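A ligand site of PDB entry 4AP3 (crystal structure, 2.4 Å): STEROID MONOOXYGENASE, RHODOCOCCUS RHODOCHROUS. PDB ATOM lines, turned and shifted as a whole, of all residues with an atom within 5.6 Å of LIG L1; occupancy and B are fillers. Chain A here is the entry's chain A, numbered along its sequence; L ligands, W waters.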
ATOM      1  N   ASP A  71      26.918  11.452 -12.898  1.00  0.00           N
ATOM      2  CA  ASP A  71      25.808  11.404 -13.871  1.00  0.00           C
ATOM      3  C   ASP A  71      25.639  12.726 -14.610  1.00  0.00           C
ATOM      4  O   ASP A  71      25.086  12.772 -15.710  1.00  0.00           O
ATOM      5  CB  ASP A  71      24.503  11.253 -13.072  1.00  0.00           C
ATOM      6  CG  ASP A  71      23.982   9.860 -13.078  1.00  0.00           C
ATOM      7  OD1 ASP A  71      24.166   9.137 -14.083  1.00  0.00           O
ATOM      8  OD2 ASP A  71      23.351   9.498 -12.058  1.00  0.00           O
ATOM      9  N   LEU A 158      21.895   9.270  -0.279  1.00  0.00           N
ATOM     10  CA  LEU A 158      22.095   7.874  -0.649  1.00  0.00           C
ATOM     11  C   LEU A 158      22.823   7.111   0.434  1.00  0.00           C
ATOM     12  O   LEU A 158      23.929   7.489   0.825  1.00  0.00           O
ATOM     13  CB  LEU A 158      22.869   7.791  -1.974  1.00  0.00           C
ATOM     14  CG  LEU A 158      22.161   7.663  -3.333  1.00  0.00           C
ATOM     15  CD1 LEU A 158      20.890   8.487  -3.470  1.00  0.00           C
ATOM     16  CD2 LEU A 158      23.148   8.048  -4.415  1.00  0.00           C
ATOM     17  N   ALA A 161      22.179   0.050   0.502  1.00  0.00           N
ATOM     18  CA  ALA A 161      21.141  -0.947   0.708  1.00  0.00           C
ATOM     19  C   ALA A 161      21.788  -2.138   1.418  1.00  0.00           C
ATOM     20  O   ALA A 161      23.002  -2.370   1.276  1.00  0.00           O
ATOM     21  CB  ALA A 161      20.499  -1.369  -0.607  1.00  0.00           C
ATOM     22  N   THR A 199      22.725  -5.506 -10.488  1.00  0.00           N
ATOM     23  CA  THR A 199      22.842  -4.810 -11.775  1.00  0.00           C
ATOM     24  C   THR A 199      22.310  -3.370 -11.692  1.00  0.00           C
ATOM     25  O   THR A 199      21.873  -2.811 -12.701  1.00  0.00           O
ATOM     26  CB  THR A 199      22.183  -5.603 -12.932  1.00  0.00           C
ATOM     27  OG1 THR A 199      20.796  -5.837 -12.653  1.00  0.00           O
ATOM     28  CG2 THR A 199      22.888  -6.936 -13.165  1.00  0.00           C
ATOM     29  N   GLY A 200      22.360  -2.780 -10.503  1.00  0.00           N
ATOM     30  CA  GLY A 200      22.142  -1.341 -10.325  1.00  0.00           C
ATOM     31  C   GLY A 200      23.358  -0.614 -10.871  1.00  0.00           C
ATOM     32  O   GLY A 200      24.191  -1.211 -11.558  1.00  0.00           O
ATOM     33  N   SER A 201      23.485   0.677 -10.563  1.00  0.00           N
ATOM     34  CA  SER A 201      24.579   1.468 -11.147  1.00  0.00           C
ATOM     35  C   SER A 201      25.966   0.985 -10.748  1.00  0.00           C
ATOM     36  O   SER A 201      26.889   1.039 -11.547  1.00  0.00           O
ATOM     37  CB  SER A 201      24.423   2.961 -10.877  1.00  0.00           C
ATOM     38  OG  SER A 201      24.179   3.180  -9.505  1.00  0.00           O
ATOM     39  N   SER A 202      26.128   0.528  -9.516  1.00  0.00           N
ATOM     40  CA  SER A 202      27.445   0.100  -9.073  1.00  0.00           C
ATOM     41  C   SER A 202      27.871  -1.146  -9.849  1.00  0.00           C
ATOM     42  O   SER A 202      29.045  -1.315 -10.172  1.00  0.00           O
ATOM     43  CB  SER A 202      27.467  -0.154  -7.580  1.00  0.00           C
ATOM     44  OG  SER A 202      26.896  -1.422  -7.309  1.00  0.00           O
ATOM     45  N   ASN A 225      17.949  -3.009 -15.612  1.00  0.00           N
ATOM     46  CA  ASN A 225      17.786  -1.560 -15.486  1.00  0.00           C
ATOM     47  C   ASN A 225      18.114  -0.815 -16.771  1.00  0.00           C
ATOM     48  O   ASN A 225      18.821  -1.331 -17.636  1.00  0.00           O
ATOM     49  CB  ASN A 225      18.636  -1.016 -14.343  1.00  0.00           C
ATOM     50  CG  ASN A 225      18.103  -1.428 -12.978  1.00  0.00           C
ATOM     51  OD1 ASN A 225      18.877  -1.770 -12.082  1.00  0.00           O
ATOM     52  ND2 ASN A 225      16.790  -1.386 -12.806  1.00  0.00           N
ATOM     53  N   LYS A 341      12.937   4.954 -12.438  1.00  0.00           N
ATOM     54  CA  LYS A 341      14.201   4.870 -11.736  1.00  0.00           C
ATOM     55  C   LYS A 341      15.191   5.698 -12.574  1.00  0.00           C
ATOM     56  O   LYS A 341      15.080   5.741 -13.804  1.00  0.00           O
ATOM     57  CB  LYS A 341      14.659   3.412 -11.623  1.00  0.00           C
ATOM     58  CG  LYS A 341      15.974   3.217 -10.873  1.00  0.00           C
ATOM     59  N   ARG A 342      16.139   6.347 -11.900  1.00  0.00           N
ATOM     60  CA  ARG A 342      17.152   7.153 -12.571  1.00  0.00           C
ATOM     61  C   ARG A 342      17.921   6.324 -13.590  1.00  0.00           C
ATOM     62  O   ARG A 342      18.342   5.192 -13.308  1.00  0.00           O
ATOM     63  CB  ARG A 342      18.112   7.757 -11.546  1.00  0.00           C
ATOM     64  CG  ARG A 342      19.052   8.817 -12.102  1.00  0.00           C
ATOM     65  CD  ARG A 342      20.005   9.280 -11.009  1.00  0.00           C
ATOM     66  NE  ARG A 342      20.858  10.389 -11.435  1.00  0.00           N
ATOM     67  CZ  ARG A 342      20.623  11.675 -11.161  1.00  0.00           C
ATOM     68  NH1 ARG A 342      19.542  12.041 -10.478  1.00  0.00           N
ATOM     69  NH2 ARG A 342      21.486  12.593 -11.571  1.00  0.00           N
ATOM     70  N   VAL A 344      20.903   4.967 -15.552  1.00  0.00           N
ATOM     71  CA  VAL A 344      22.328   4.767 -15.284  1.00  0.00           C
ATOM     72  C   VAL A 344      23.162   5.270 -16.465  1.00  0.00           C
ATOM     73  O   VAL A 344      22.696   5.260 -17.610  1.00  0.00           O
ATOM     74  CB  VAL A 344      22.643   3.281 -14.966  1.00  0.00           C
ATOM     75  CG1 VAL A 344      24.130   3.063 -14.706  1.00  0.00           C
ATOM     76  CG2 VAL A 344      21.823   2.821 -13.771  1.00  0.00           C
ATOM     77  N   ALA A 391      27.498  -6.196  -5.797  1.00  0.00           N
ATOM     78  CA  ALA A 391      27.314  -4.840  -6.298  1.00  0.00           C
ATOM     79  C   ALA A 391      26.007  -4.289  -5.741  1.00  0.00           C
ATOM     80  O   ALA A 391      24.947  -4.459  -6.343  1.00  0.00           O
ATOM     81  CB  ALA A 391      27.332  -4.821  -7.815  1.00  0.00           C
ATOM     82  N   THR A 392      26.097  -3.655  -4.575  1.00  0.00           N
ATOM     83  CA  THR A 392      24.894  -3.258  -3.836  1.00  0.00           C
ATOM     84  C   THR A 392      24.273  -1.966  -4.327  1.00  0.00           C
ATOM     85  O   THR A 392      24.929  -1.150  -4.987  1.00  0.00           O
ATOM     86  CB  THR A 392      25.172  -3.136  -2.328  1.00  0.00           C
ATOM     87  OG1 THR A 392      26.454  -2.531  -2.130  1.00  0.00           O
ATOM     88  CG2 THR A 392      25.141  -4.507  -1.671  1.00  0.00           C
ATOM     89  N   GLY A 393      22.996  -1.792  -3.997  1.00  0.00           N
ATOM     90  CA  GLY A 393      22.280  -0.573  -4.323  1.00  0.00           C
ATOM     91  C   GLY A 393      22.245   0.451  -3.209  1.00  0.00           C
ATOM     92  O   GLY A 393      22.922   0.307  -2.185  1.00  0.00           O
ATOM     93  N   PHE A 394      21.444   1.489  -3.396  1.00  0.00           N
ATOM     94  CA  PHE A 394      21.348   2.582  -2.446  1.00  0.00           C
ATOM     95  C   PHE A 394      19.922   2.814  -2.046  1.00  0.00           C
ATOM     96  O   PHE A 394      19.027   2.866  -2.900  1.00  0.00           O
ATOM     97  CB  PHE A 394      21.923   3.868  -3.060  1.00  0.00           C
ATOM     98  CG  PHE A 394      23.313   3.704  -3.604  1.00  0.00           C
ATOM     99  CD1 PHE A 394      23.506   3.281  -4.902  1.00  0.00           C
ATOM    100  CD2 PHE A 394      24.421   3.956  -2.797  1.00  0.00           C
ATOM    101  CE1 PHE A 394      24.789   3.112  -5.404  1.00  0.00           C
ATOM    102  CE2 PHE A 394      25.703   3.786  -3.299  1.00  0.00           C
ATOM    103  CZ  PHE A 394      25.885   3.369  -4.602  1.00  0.00           C
ATOM    104  N   VAL A 447      17.650  14.583  -4.877  1.00  0.00           N
ATOM    105  CA  VAL A 447      18.367  13.894  -5.968  1.00  0.00           C
ATOM    106  C   VAL A 447      17.826  14.196  -7.376  1.00  0.00           C
ATOM    107  O   VAL A 447      18.480  13.867  -8.370  1.00  0.00           O
ATOM    108  CB  VAL A 447      18.405  12.354  -5.770  1.00  0.00           C
ATOM    109  CG1 VAL A 447      19.115  12.005  -4.483  1.00  0.00           C
ATOM    110  CG2 VAL A 447      17.005  11.750  -5.766  1.00  0.00           C
ATOM    111  N   TRP A 506      11.649   4.247  -6.549  1.00  0.00           N
ATOM    112  CA  TRP A 506      12.829   4.668  -5.810  1.00  0.00           C
ATOM    113  C   TRP A 506      12.556   5.788  -4.836  1.00  0.00           C
ATOM    114  O   TRP A 506      13.147   5.844  -3.763  1.00  0.00           O
ATOM    115  CB  TRP A 506      13.875   5.113  -6.827  1.00  0.00           C
ATOM    116  CG  TRP A 506      15.286   4.693  -6.526  1.00  0.00           C
ATOM    117  CD1 TRP A 506      15.774   3.398  -6.358  1.00  0.00           C
ATOM    118  CD2 TRP A 506      16.460   5.569  -6.396  1.00  0.00           C
ATOM    119  NE1 TRP A 506      17.125   3.410  -6.112  1.00  0.00           N
ATOM    120  CE2 TRP A 506      17.598   4.681  -6.132  1.00  0.00           C
ATOM    121  CE3 TRP A 506      16.673   6.939  -6.467  1.00  0.00           C
ATOM    122  CZ2 TRP A 506      18.886   5.171  -5.941  1.00  0.00           C
ATOM    123  CZ3 TRP A 506      17.971   7.426  -6.285  1.00  0.00           C
ATOM    124  CH2 TRP A 506      19.046   6.559  -6.027  1.00  0.00           C
HETATM  125  P1  LIG L   1      19.545  -0.946  -7.098  1.00  0.00           P
HETATM  126  O1  LIG L   1      20.149  -2.425  -6.956  1.00  0.00           O
HETATM  127  O2  LIG L   1      18.730  -0.883  -8.373  1.00  0.00           O
HETATM  128  O3  LIG L   1      18.911  -0.554  -5.785  1.00  0.00           O
HETATM  129  O4  LIG L   1      20.886  -0.058  -7.300  1.00  0.00           O
HETATM  130  P2  LIG L   1      20.824   1.515  -7.613  1.00  0.00           P
HETATM  131  O5  LIG L   1      20.054   1.707  -8.903  1.00  0.00           O
HETATM  132  O6  LIG L   1      22.213   2.090  -7.514  1.00  0.00           O
HETATM  133  O7  LIG L   1      19.948   2.059  -6.372  1.00  0.00           O
HETATM  134  N1  LIG L   1      22.249   6.187  -7.878  1.00  0.00           N
HETATM  135  C1  LIG L   1      21.832   7.465  -7.716  1.00  0.00           C
HETATM  136  C2  LIG L   1      22.512   8.519  -8.342  1.00  0.00           C
HETATM  137  C3  LIG L   1      22.051   9.931  -8.146  1.00  0.00           C
HETATM  138  O8  LIG L   1      21.228  10.206  -7.288  1.00  0.00           O
HETATM  139  N2  LIG L   1      22.570  10.880  -8.925  1.00  0.00           N
HETATM  140  C4  LIG L   1      23.623   8.232  -9.135  1.00  0.00           C
HETATM  141  C5  LIG L   1      24.033   6.911  -9.290  1.00  0.00           C
HETATM  142  C6  LIG L   1      23.311   5.897  -8.639  1.00  0.00           C
HETATM  143  P1  LG2 L   2      27.197  12.592   0.927  1.00  0.00           P
HETATM  144  O1  LG2 L   2      28.180  12.709  -0.210  1.00  0.00           O
HETATM  145  O2  LG2 L   2      26.497  11.285   1.106  1.00  0.00           O
HETATM  146  O3  LG2 L   2      27.928  12.976   2.287  1.00  0.00           O
HETATM  147  C1  LG2 L   2      27.272  12.717   3.529  1.00  0.00           C
HETATM  148  C2  LG2 L   2      28.306  12.374   4.581  1.00  0.00           C
HETATM  149  O4  LG2 L   2      27.667  12.340   5.840  1.00  0.00           O
HETATM  150  C3  LG2 L   2      28.913  10.982   4.386  1.00  0.00           C
HETATM  151  O5  LG2 L   2      30.334  11.109   4.475  1.00  0.00           O
HETATM  152  C4  LG2 L   2      28.455  10.172   5.588  1.00  0.00           C
HETATM  153  O6  LG2 L   2      29.516   9.311   6.049  1.00  0.00           O
HETATM  154  C5  LG2 L   2      28.203  11.267   6.621  1.00  0.00           C
HETATM  155  N1  LG2 L   2      27.270  10.850   7.679  1.00  0.00           N
HETATM  156  C6  LG2 L   2      26.030  10.334   7.524  1.00  0.00           C
HETATM  157  N2  LG2 L   2      25.464  10.082   8.725  1.00  0.00           N
HETATM  158  C7  LG2 L   2      26.353  10.404   9.675  1.00  0.00           C
HETATM  159  C8  LG2 L   2      26.385  10.390  11.146  1.00  0.00           C
HETATM  160  N3  LG2 L   2      25.339   9.940  11.860  1.00  0.00           N
HETATM  161  N4  LG2 L   2      27.511  10.838  11.772  1.00  0.00           N
HETATM  162  C9  LG2 L   2      28.562  11.280  11.055  1.00  0.00           C
HETATM  163  N5  LG2 L   2      28.571  11.340   9.712  1.00  0.00           N
HETATM  164  C10 LG2 L   2      27.531  10.922   8.985  1.00  0.00           C
HETATM  165  N6  LG2 L   2      24.260  13.524  -7.655  1.00  0.00           N
HETATM  166  C11 LG2 L   2      24.166  14.502  -8.590  1.00  0.00           C
HETATM  167  O7  LG2 L   2      23.513  15.536  -8.327  1.00  0.00           O
HETATM  168  N7  LG2 L   2      24.763  14.413  -9.796  1.00  0.00           N
HETATM  169  C12 LG2 L   2      25.490  13.348 -10.142  1.00  0.00           C
HETATM  170  O8  LG2 L   2      26.054  13.278 -11.256  1.00  0.00           O
HETATM  171  C13 LG2 L   2      25.631  12.226  -9.185  1.00  0.00           C
HETATM  172  N8  LG2 L   2      26.347  11.122  -9.494  1.00  0.00           N
HETATM  173  C14 LG2 L   2      26.465  10.120  -8.601  1.00  0.00           C
HETATM  174  C15 LG2 L   2      27.199   8.991  -8.958  1.00  0.00           C
HETATM  175  C16 LG2 L   2      27.356   7.929  -8.064  1.00  0.00           C
HETATM  176  C17 LG2 L   2      28.176   6.732  -8.475  1.00  0.00           C
HETATM  177  C18 LG2 L   2      26.704   8.014  -6.725  1.00  0.00           C
HETATM  178  C19 LG2 L   2      26.831   6.899  -5.731  1.00  0.00           C
HETATM  179  C20 LG2 L   2      25.964   9.142  -6.375  1.00  0.00           C
HETATM  180  C21 LG2 L   2      25.814  10.206  -7.262  1.00  0.00           C
HETATM  181  N9  LG2 L   2      25.056  11.361  -6.920  1.00  0.00           N
HETATM  182  C22 LG2 L   2      24.957  12.390  -7.881  1.00  0.00           C
HETATM  183  C23 LG2 L   2      24.346  11.518  -5.637  1.00  0.00           C
HETATM  184  C24 LG2 L   2      25.246  11.872  -4.473  1.00  0.00           C
HETATM  185  O9  LG2 L   2      24.748  11.121  -3.380  1.00  0.00           O
HETATM  186  C25 LG2 L   2      25.146  13.351  -4.137  1.00  0.00           C
HETATM  187  O10 LG2 L   2      25.418  14.098  -5.317  1.00  0.00           O
HETATM  188  C26 LG2 L   2      26.086  13.754  -3.025  1.00  0.00           C
HETATM  189  O11 LG2 L   2      26.343  12.639  -2.147  1.00  0.00           O
HETATM  190  C27 LG2 L   2      25.475  14.850  -2.156  1.00  0.00           C
HETATM  191  O12 LG2 L   2      26.475  15.194  -1.203  1.00  0.00           O
HETATM  192  P2  LG2 L   2      26.163  15.268   0.350  1.00  0.00           P
HETATM  193  O13 LG2 L   2      27.313  15.952   1.067  1.00  0.00           O
HETATM  194  O14 LG2 L   2      24.778  15.842   0.470  1.00  0.00           O
HETATM  195  O15 LG2 L   2      26.031  13.725   0.838  1.00  0.00           O
HETATM  196  O   HOH W   1      24.198   0.049  -7.561  1.00  0.00           O
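OD2 of Asp 71 lies within salt-bridge range of NE of Arg 342.
NH1 of Arg 342 sits at hydrogen-bond distance from O of Val 447 (3.0 Å).
The backbone carbonyl oxygen (O) of Gly 393 sits at hydrogen-bond distance from the backbone NH (N) of Ala 161 (2.8 Å).
OD1 of Asn 225 sits close to O of Thr 199, at 3.2 Å.
Water W1 lies within hydrogen-bond range of the backbone NH of Ser 202 (2.8 Å), an oxygen (O6) of LIG L1 (2.8 Å), the backbone carbonyl oxygen of Thr 392 (2.9 Å) and the backbone NH of Ser 201 (3.1 Å).
The side-chain hydroxyl of Ser 201 lies close to an oxygen (O6) of LIG L1.
O7 of LIG L1 lies within hydrogen-bond range of NE1 of Trp 506, 3.1 Å away.
The backbone NH of Phe 394 sits at hydrogen-bond distance from an oxygen (O7) of LIG L1 (3.4 Å).
The backbone NH (N) of Asp 71 is in hydrogen-bond range of an oxygen (O8) of LG2 L2 (2.6 Å).
A nitrogen (N2) of LIG L1 lies close to a nitrogen (N6) of LG2 L2, at 3.4 Å.
The guanidinium group of Arg 342 lies close to a nitrogen (N2) of LIG L1, at 3.1 Å.
Merely in contact with LIG L1: Asp 71, Gly 393, Gly 200, Leu 158, Asn 225 and Val 447.
Within 4 Å of LIG L1: Asp 71, Leu 158, Gly 200, Ser 201, Asn 225, Arg 342, Gly 393, Phe 394, Val 447 and Trp 506.
The nearest printed residue that does not touch LIG L1 is Ser 202 (4.7 Å).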
